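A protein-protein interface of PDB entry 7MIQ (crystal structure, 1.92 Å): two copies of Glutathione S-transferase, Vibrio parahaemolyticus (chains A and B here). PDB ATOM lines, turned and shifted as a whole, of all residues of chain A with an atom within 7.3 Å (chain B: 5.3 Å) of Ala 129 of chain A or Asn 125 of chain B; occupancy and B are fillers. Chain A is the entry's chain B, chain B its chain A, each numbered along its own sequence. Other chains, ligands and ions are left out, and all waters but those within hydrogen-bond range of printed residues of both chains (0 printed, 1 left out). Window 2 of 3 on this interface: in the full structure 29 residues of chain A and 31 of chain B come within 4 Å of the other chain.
1 position is printed for both chains.
Of the 8 pairs that touch across the chains among the printed residues, none has its exchanged pair printed and touching as well.
The backbone NH (N) of Ala 129 of chain A sits close to the backbone carbonyl oxygen (O) of Asp 122 of chain B.
O of Asp 122 of chain B lies within hydrogen-bond range of N of Trp 130 of chain A (2.9 Å).
The backbone NH (N) of Ala 128 of chain A lies close to the backbone NH (N) of Glu 124 of chain B (3.3 Å).
Of the printed residues of chain B, Ala 128 of chain A touches Arg 123 (3.2 Å) and Glu 124 (3.3 Å).
Printed residues of chain B within 4 Å of Glu 133 of chain A: Gln 121 (3.5 Å).
Of the printed residues of chain A, Asp 122 of chain B touches Ala 129 and Trp 130.
Printed residues of chain B that touch a printed residue of chain A: Gln 121, Asp 122, Arg 123, Glu 124 and Asn 125.
Along chain B the printed residues that touch a printed residue of chain A span positions 121 to 125.
Printed residues of chain A that touch a printed residue of chain B: Ala 128, Ala 129, Trp 130 and Glu 133.
Among the printed residues, 8 pairs touch across the chains.
Among the printed residues, no Asp or Glu carboxylate lies within 4 Å of a Lys or Arg side-chain nitrogen of the other chain.
Among the printed residues, pairs that only touch across the chains: Ala 128 of chain A with Arg 123 of chain B (3.2 Å), Ala 129 of chain A with Glu 124 of chain B (3.5 Å), Ala 129 of chain A with Asn 125 of chain B (3.7 Å), Trp 130 of chain A with Gln 121 of chain B (3.0 Å) and Glu 133 of chain A with Gln 121 of chain B (3.5 Å).
The backbone carbonyl oxygen (O) of Cys 126 of chain B sits at hydrogen-bond distance from the backbone NH (N) of Gln 121 of chain B, at 3.0 Å.
ND2 of Asn 125 of chain B is in hydrogen-bond range of O of Arg 123 of chain B (3.4 Å).
The backbone carbonyl oxygen (O) of Trp 130 of chain A sits at hydrogen-bond distance from the side-chain hydroxyl (OG) of Ser 134 of chain A (2.9 Å).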
ATOM      1  N   ASN A 115     -25.185  -9.280 -16.756  1.00  0.00           N
ATOM      2  CA  ASN A 115     -23.811  -9.028 -17.172  1.00  0.00           C
ATOM      3  C   ASN A 115     -23.662  -9.204 -18.681  1.00  0.00           C
ATOM      4  O   ASN A 115     -22.778  -9.923 -19.148  1.00  0.00           O
ATOM      5  CB  ASN A 115     -22.840  -9.957 -16.439  1.00  0.00           C
ATOM      6  CG  ASN A 115     -22.861  -9.758 -14.935  1.00  0.00           C
ATOM      7  OD1 ASN A 115     -23.448  -8.801 -14.431  1.00  0.00           O
ATOM      8  ND2 ASN A 115     -22.205 -10.658 -14.210  1.00  0.00           N
ATOM      9  N   ALA A 128     -17.887  -8.951 -17.321  1.00  0.00           N
ATOM     10  CA  ALA A 128     -18.112  -9.945 -18.359  1.00  0.00           C
ATOM     11  C   ALA A 128     -17.615 -11.320 -17.923  1.00  0.00           C
ATOM     12  O   ALA A 128     -18.222 -12.338 -18.253  1.00  0.00           O
ATOM     13  CB  ALA A 128     -17.436  -9.520 -19.655  1.00  0.00           C
ATOM     14  N   ALA A 129     -16.507 -11.348 -17.177  1.00  0.00           N
ATOM     15  CA  ALA A 129     -15.926 -12.626 -16.779  1.00  0.00           C
ATOM     16  C   ALA A 129     -16.821 -13.376 -15.797  1.00  0.00           C
ATOM     17  O   ALA A 129     -16.877 -14.611 -15.838  1.00  0.00           O
ATOM     18  CB  ALA A 129     -14.535 -12.413 -16.181  1.00  0.00           C
ATOM     19  N   TRP A 130     -17.521 -12.662 -14.912  1.00  0.00           N
ATOM     20  CA  TRP A 130     -18.457 -13.337 -14.017  1.00  0.00           C
ATOM     21  C   TRP A 130     -19.736 -13.724 -14.745  1.00  0.00           C
ATOM     22  O   TRP A 130     -20.303 -14.789 -14.482  1.00  0.00           O
ATOM     23  CB  TRP A 130     -18.785 -12.456 -12.813  1.00  0.00           C
ATOM     24  CG  TRP A 130     -19.700 -13.100 -11.800  1.00  0.00           C
ATOM     25  CD1 TRP A 130     -20.857 -12.577 -11.297  1.00  0.00           C
ATOM     26  CD2 TRP A 130     -19.535 -14.383 -11.172  1.00  0.00           C
ATOM     27  NE1 TRP A 130     -21.420 -13.449 -10.396  1.00  0.00           N
ATOM     28  CE2 TRP A 130     -20.629 -14.564 -10.302  1.00  0.00           C
ATOM     29  CE3 TRP A 130     -18.572 -15.394 -11.262  1.00  0.00           C
ATOM     30  CZ2 TRP A 130     -20.786 -15.714  -9.528  1.00  0.00           C
ATOM     31  CZ3 TRP A 130     -18.729 -16.533 -10.491  1.00  0.00           C
ATOM     32  CH2 TRP A 130     -19.826 -16.683  -9.637  1.00  0.00           C
ATOM     33  N   GLY A 131     -20.209 -12.866 -15.650  1.00  0.00           N
ATOM     34  CA  GLY A 131     -21.358 -13.229 -16.460  1.00  0.00           C
ATOM     35  C   GLY A 131     -21.091 -14.447 -17.319  1.00  0.00           C
ATOM     36  O   GLY A 131     -21.956 -15.313 -17.473  1.00  0.00           O
ATOM     37  N   GLU A 132     -19.883 -14.536 -17.885  1.00  0.00           N
ATOM     38  CA  GLU A 132     -19.513 -15.711 -18.666  1.00  0.00           C
ATOM     39  C   GLU A 132     -19.395 -16.944 -17.783  1.00  0.00           C
ATOM     40  O   GLU A 132     -19.791 -18.044 -18.186  1.00  0.00           O
ATOM     41  CB  GLU A 132     -18.205 -15.456 -19.415  1.00  0.00           C
ATOM     42  CG  GLU A 132     -18.392 -15.163 -20.892  1.00  0.00           C
ATOM     43  CD  GLU A 132     -19.001 -16.334 -21.638  1.00  0.00           C
ATOM     44  OE1 GLU A 132     -18.634 -17.488 -21.334  1.00  0.00           O
ATOM     45  OE2 GLU A 132     -19.852 -16.102 -22.522  1.00  0.00           O
ATOM     46  N   GLU A 133     -18.845 -16.783 -16.578  1.00  0.00           N
ATOM     47  CA  GLU A 133     -18.791 -17.897 -15.639  1.00  0.00           C
ATOM     48  C   GLU A 133     -20.191 -18.326 -15.220  1.00  0.00           C
ATOM     49  O   GLU A 133     -20.480 -19.524 -15.121  1.00  0.00           O
ATOM     50  CB  GLU A 133     -17.953 -17.513 -14.417  1.00  0.00           C
ATOM     51  CG  GLU A 133     -17.901 -18.573 -13.331  1.00  0.00           C
ATOM     52  CD  GLU A 133     -17.156 -19.820 -13.763  1.00  0.00           C
ATOM     53  OE1 GLU A 133     -16.314 -19.725 -14.681  1.00  0.00           O
ATOM     54  OE2 GLU A 133     -17.415 -20.898 -13.186  1.00  0.00           O
ATOM     55  N   SER A 134     -21.076 -17.356 -14.976  1.00  0.00           N
ATOM     56  CA  SER A 134     -22.454 -17.681 -14.625  1.00  0.00           C
ATOM     57  C   SER A 134     -23.155 -18.406 -15.768  1.00  0.00           C
ATOM     58  O   SER A 134     -23.918 -19.351 -15.536  1.00  0.00           O
ATOM     59  CB  SER A 134     -23.214 -16.412 -14.248  1.00  0.00           C
ATOM     60  OG  SER A 134     -22.651 -15.803 -13.099  1.00  0.00           O
ATOM     61  N   LYS A 135     -22.902 -17.985 -17.010  1.00  0.00           N
ATOM     62  CA  LYS A 135     -23.500 -18.671 -18.150  1.00  0.00           C
ATOM     63  C   LYS A 135     -23.010 -20.109 -18.244  1.00  0.00           C
ATOM     64  O   LYS A 135     -23.790 -21.019 -18.549  1.00  0.00           O
ATOM     65  CB  LYS A 135     -23.199 -17.914 -19.444  1.00  0.00           C
ATOM     66  CG  LYS A 135     -23.836 -18.541 -20.678  1.00  0.00           C
ATOM     67  CD  LYS A 135     -23.715 -17.638 -21.890  1.00  0.00           C
ATOM     68  CE  LYS A 135     -24.428 -18.237 -23.090  1.00  0.00           C
ATOM     69  NZ  LYS A 135     -24.434 -17.307 -24.252  1.00  0.00           N
ATOM     70  N   GLN B 121     -13.361 -13.824 -12.013  1.00  0.00           N
ATOM     71  CA  GLN B 121     -14.759 -14.205 -11.867  1.00  0.00           C
ATOM     72  C   GLN B 121     -15.618 -13.042 -11.372  1.00  0.00           C
ATOM     73  O   GLN B 121     -16.590 -13.242 -10.648  1.00  0.00           O
ATOM     74  CB  GLN B 121     -14.891 -15.402 -10.924  1.00  0.00           C
ATOM     75  CG  GLN B 121     -14.971 -16.742 -11.643  1.00  0.00           C
ATOM     76  CD  GLN B 121     -13.814 -16.967 -12.599  1.00  0.00           C
ATOM     77  OE1 GLN B 121     -12.659 -17.061 -12.185  1.00  0.00           O
ATOM     78  NE2 GLN B 121     -14.120 -17.052 -13.889  1.00  0.00           N
ATOM     79  N   ASP B 122     -15.243 -11.823 -11.754  1.00  0.00           N
ATOM     80  CA  ASP B 122     -16.136 -10.677 -11.631  1.00  0.00           C
ATOM     81  C   ASP B 122     -16.233 -10.011 -12.998  1.00  0.00           C
ATOM     82  O   ASP B 122     -15.738 -10.563 -13.985  1.00  0.00           O
ATOM     83  CB  ASP B 122     -15.654  -9.700 -10.558  1.00  0.00           C
ATOM     84  CG  ASP B 122     -16.783  -8.845 -10.002  1.00  0.00           C
ATOM     85  OD1 ASP B 122     -17.923  -8.967 -10.500  1.00  0.00           O
ATOM     86  OD2 ASP B 122     -16.533  -8.057  -9.065  1.00  0.00           O
ATOM     87  N   ARG B 123     -16.869  -8.846 -13.088  1.00  0.00           N
ATOM     88  CA  ARG B 123     -16.997  -8.170 -14.377  1.00  0.00           C
ATOM     89  C   ARG B 123     -15.616  -7.721 -14.837  1.00  0.00           C
ATOM     90  O   ARG B 123     -15.062  -6.745 -14.328  1.00  0.00           O
ATOM     91  CB  ARG B 123     -17.977  -7.002 -14.288  1.00  0.00           C
ATOM     92  CG  ARG B 123     -17.780  -6.053 -13.111  1.00  0.00           C
ATOM     93  CD  ARG B 123     -17.304  -4.680 -13.577  1.00  0.00           C
ATOM     94  NE  ARG B 123     -15.882  -4.675 -13.904  1.00  0.00           N
ATOM     95  CZ  ARG B 123     -15.244  -3.664 -14.475  1.00  0.00           C
ATOM     96  NH1 ARG B 123     -15.875  -2.554 -14.823  1.00  0.00           N
ATOM     97  NH2 ARG B 123     -13.938  -3.767 -14.704  1.00  0.00           N
ATOM     98  N   GLU B 124     -15.047  -8.445 -15.802  1.00  0.00           N
ATOM     99  CA  GLU B 124     -13.685  -8.201 -16.276  1.00  0.00           C
ATOM    100  C   GLU B 124     -12.712  -8.138 -15.094  1.00  0.00           C
ATOM    101  O   GLU B 124     -12.205  -7.084 -14.707  1.00  0.00           O
ATOM    102  CB  GLU B 124     -13.633  -6.929 -17.132  1.00  0.00           C
ATOM    103  CG  GLU B 124     -12.250  -6.583 -17.678  1.00  0.00           C
ATOM    104  CD  GLU B 124     -11.444  -7.810 -18.060  1.00  0.00           C
ATOM    105  OE1 GLU B 124     -11.888  -8.566 -18.952  1.00  0.00           O
ATOM    106  OE2 GLU B 124     -10.372  -8.026 -17.457  1.00  0.00           O
ATOM    107  N   ASN B 125     -12.492  -9.314 -14.510  1.00  0.00           N
ATOM    108  CA  ASN B 125     -11.671  -9.455 -13.313  1.00  0.00           C
ATOM    109  C   ASN B 125     -11.304 -10.924 -13.151  1.00  0.00           C
ATOM    110  O   ASN B 125     -11.699 -11.777 -13.950  1.00  0.00           O
ATOM    111  CB  ASN B 125     -12.402  -8.927 -12.075  1.00  0.00           C
ATOM    112  CG  ASN B 125     -12.142  -7.454 -11.824  1.00  0.00           C
ATOM    113  OD1 ASN B 125     -11.017  -6.975 -11.976  1.00  0.00           O
ATOM    114  ND2 ASN B 125     -13.185  -6.725 -11.441  1.00  0.00           N
ATOM    115  N   CYS B 126     -10.540 -11.215 -12.100  1.00  0.00           N
ATOM    116  CA  CYS B 126     -10.155 -12.573 -11.753  1.00  0.00           C
ATOM    117  C   CYS B 126     -10.909 -13.012 -10.497  1.00  0.00           C
ATOM    118  O   CYS B 126     -11.796 -12.309 -10.001  1.00  0.00           O
ATOM    119  CB  CYS B 126      -8.638 -12.667 -11.574  1.00  0.00           C
ATOM    120  SG  CYS B 126      -8.008 -11.903 -10.064  1.00  0.00           S
ATOM    121  N   VAL B 127     -10.552 -14.192  -9.983  1.00  0.00           N
ATOM    122  CA  VAL B 127     -11.289 -14.775  -8.866  1.00  0.00           C
ATOM    123  C   VAL B 127     -11.156 -13.918  -7.614  1.00  0.00           C
ATOM    124  O   VAL B 127     -12.095 -13.825  -6.814  1.00  0.00           O
ATOM    125  CB  VAL B 127     -10.813 -16.218  -8.605  1.00  0.00           C
ATOM    126  CG1 VAL B 127     -11.881 -17.006  -7.861  1.00  0.00           C
ATOM    127  CG2 VAL B 127     -10.437 -16.902  -9.909  1.00  0.00           C
ATOM    128  N   ALA B 129     -10.979 -10.659  -7.266  1.00  0.00           N
ATOM    129  CA  ALA B 129     -11.861  -9.499  -7.253  1.00  0.00           C
ATOM    130  C   ALA B 129     -13.298  -9.886  -6.932  1.00  0.00           C
ATOM    131  O   ALA B 129     -14.034  -9.089  -6.340  1.00  0.00           O
ATOM    132  CB  ALA B 129     -11.792  -8.770  -8.592  1.00  0.00           C
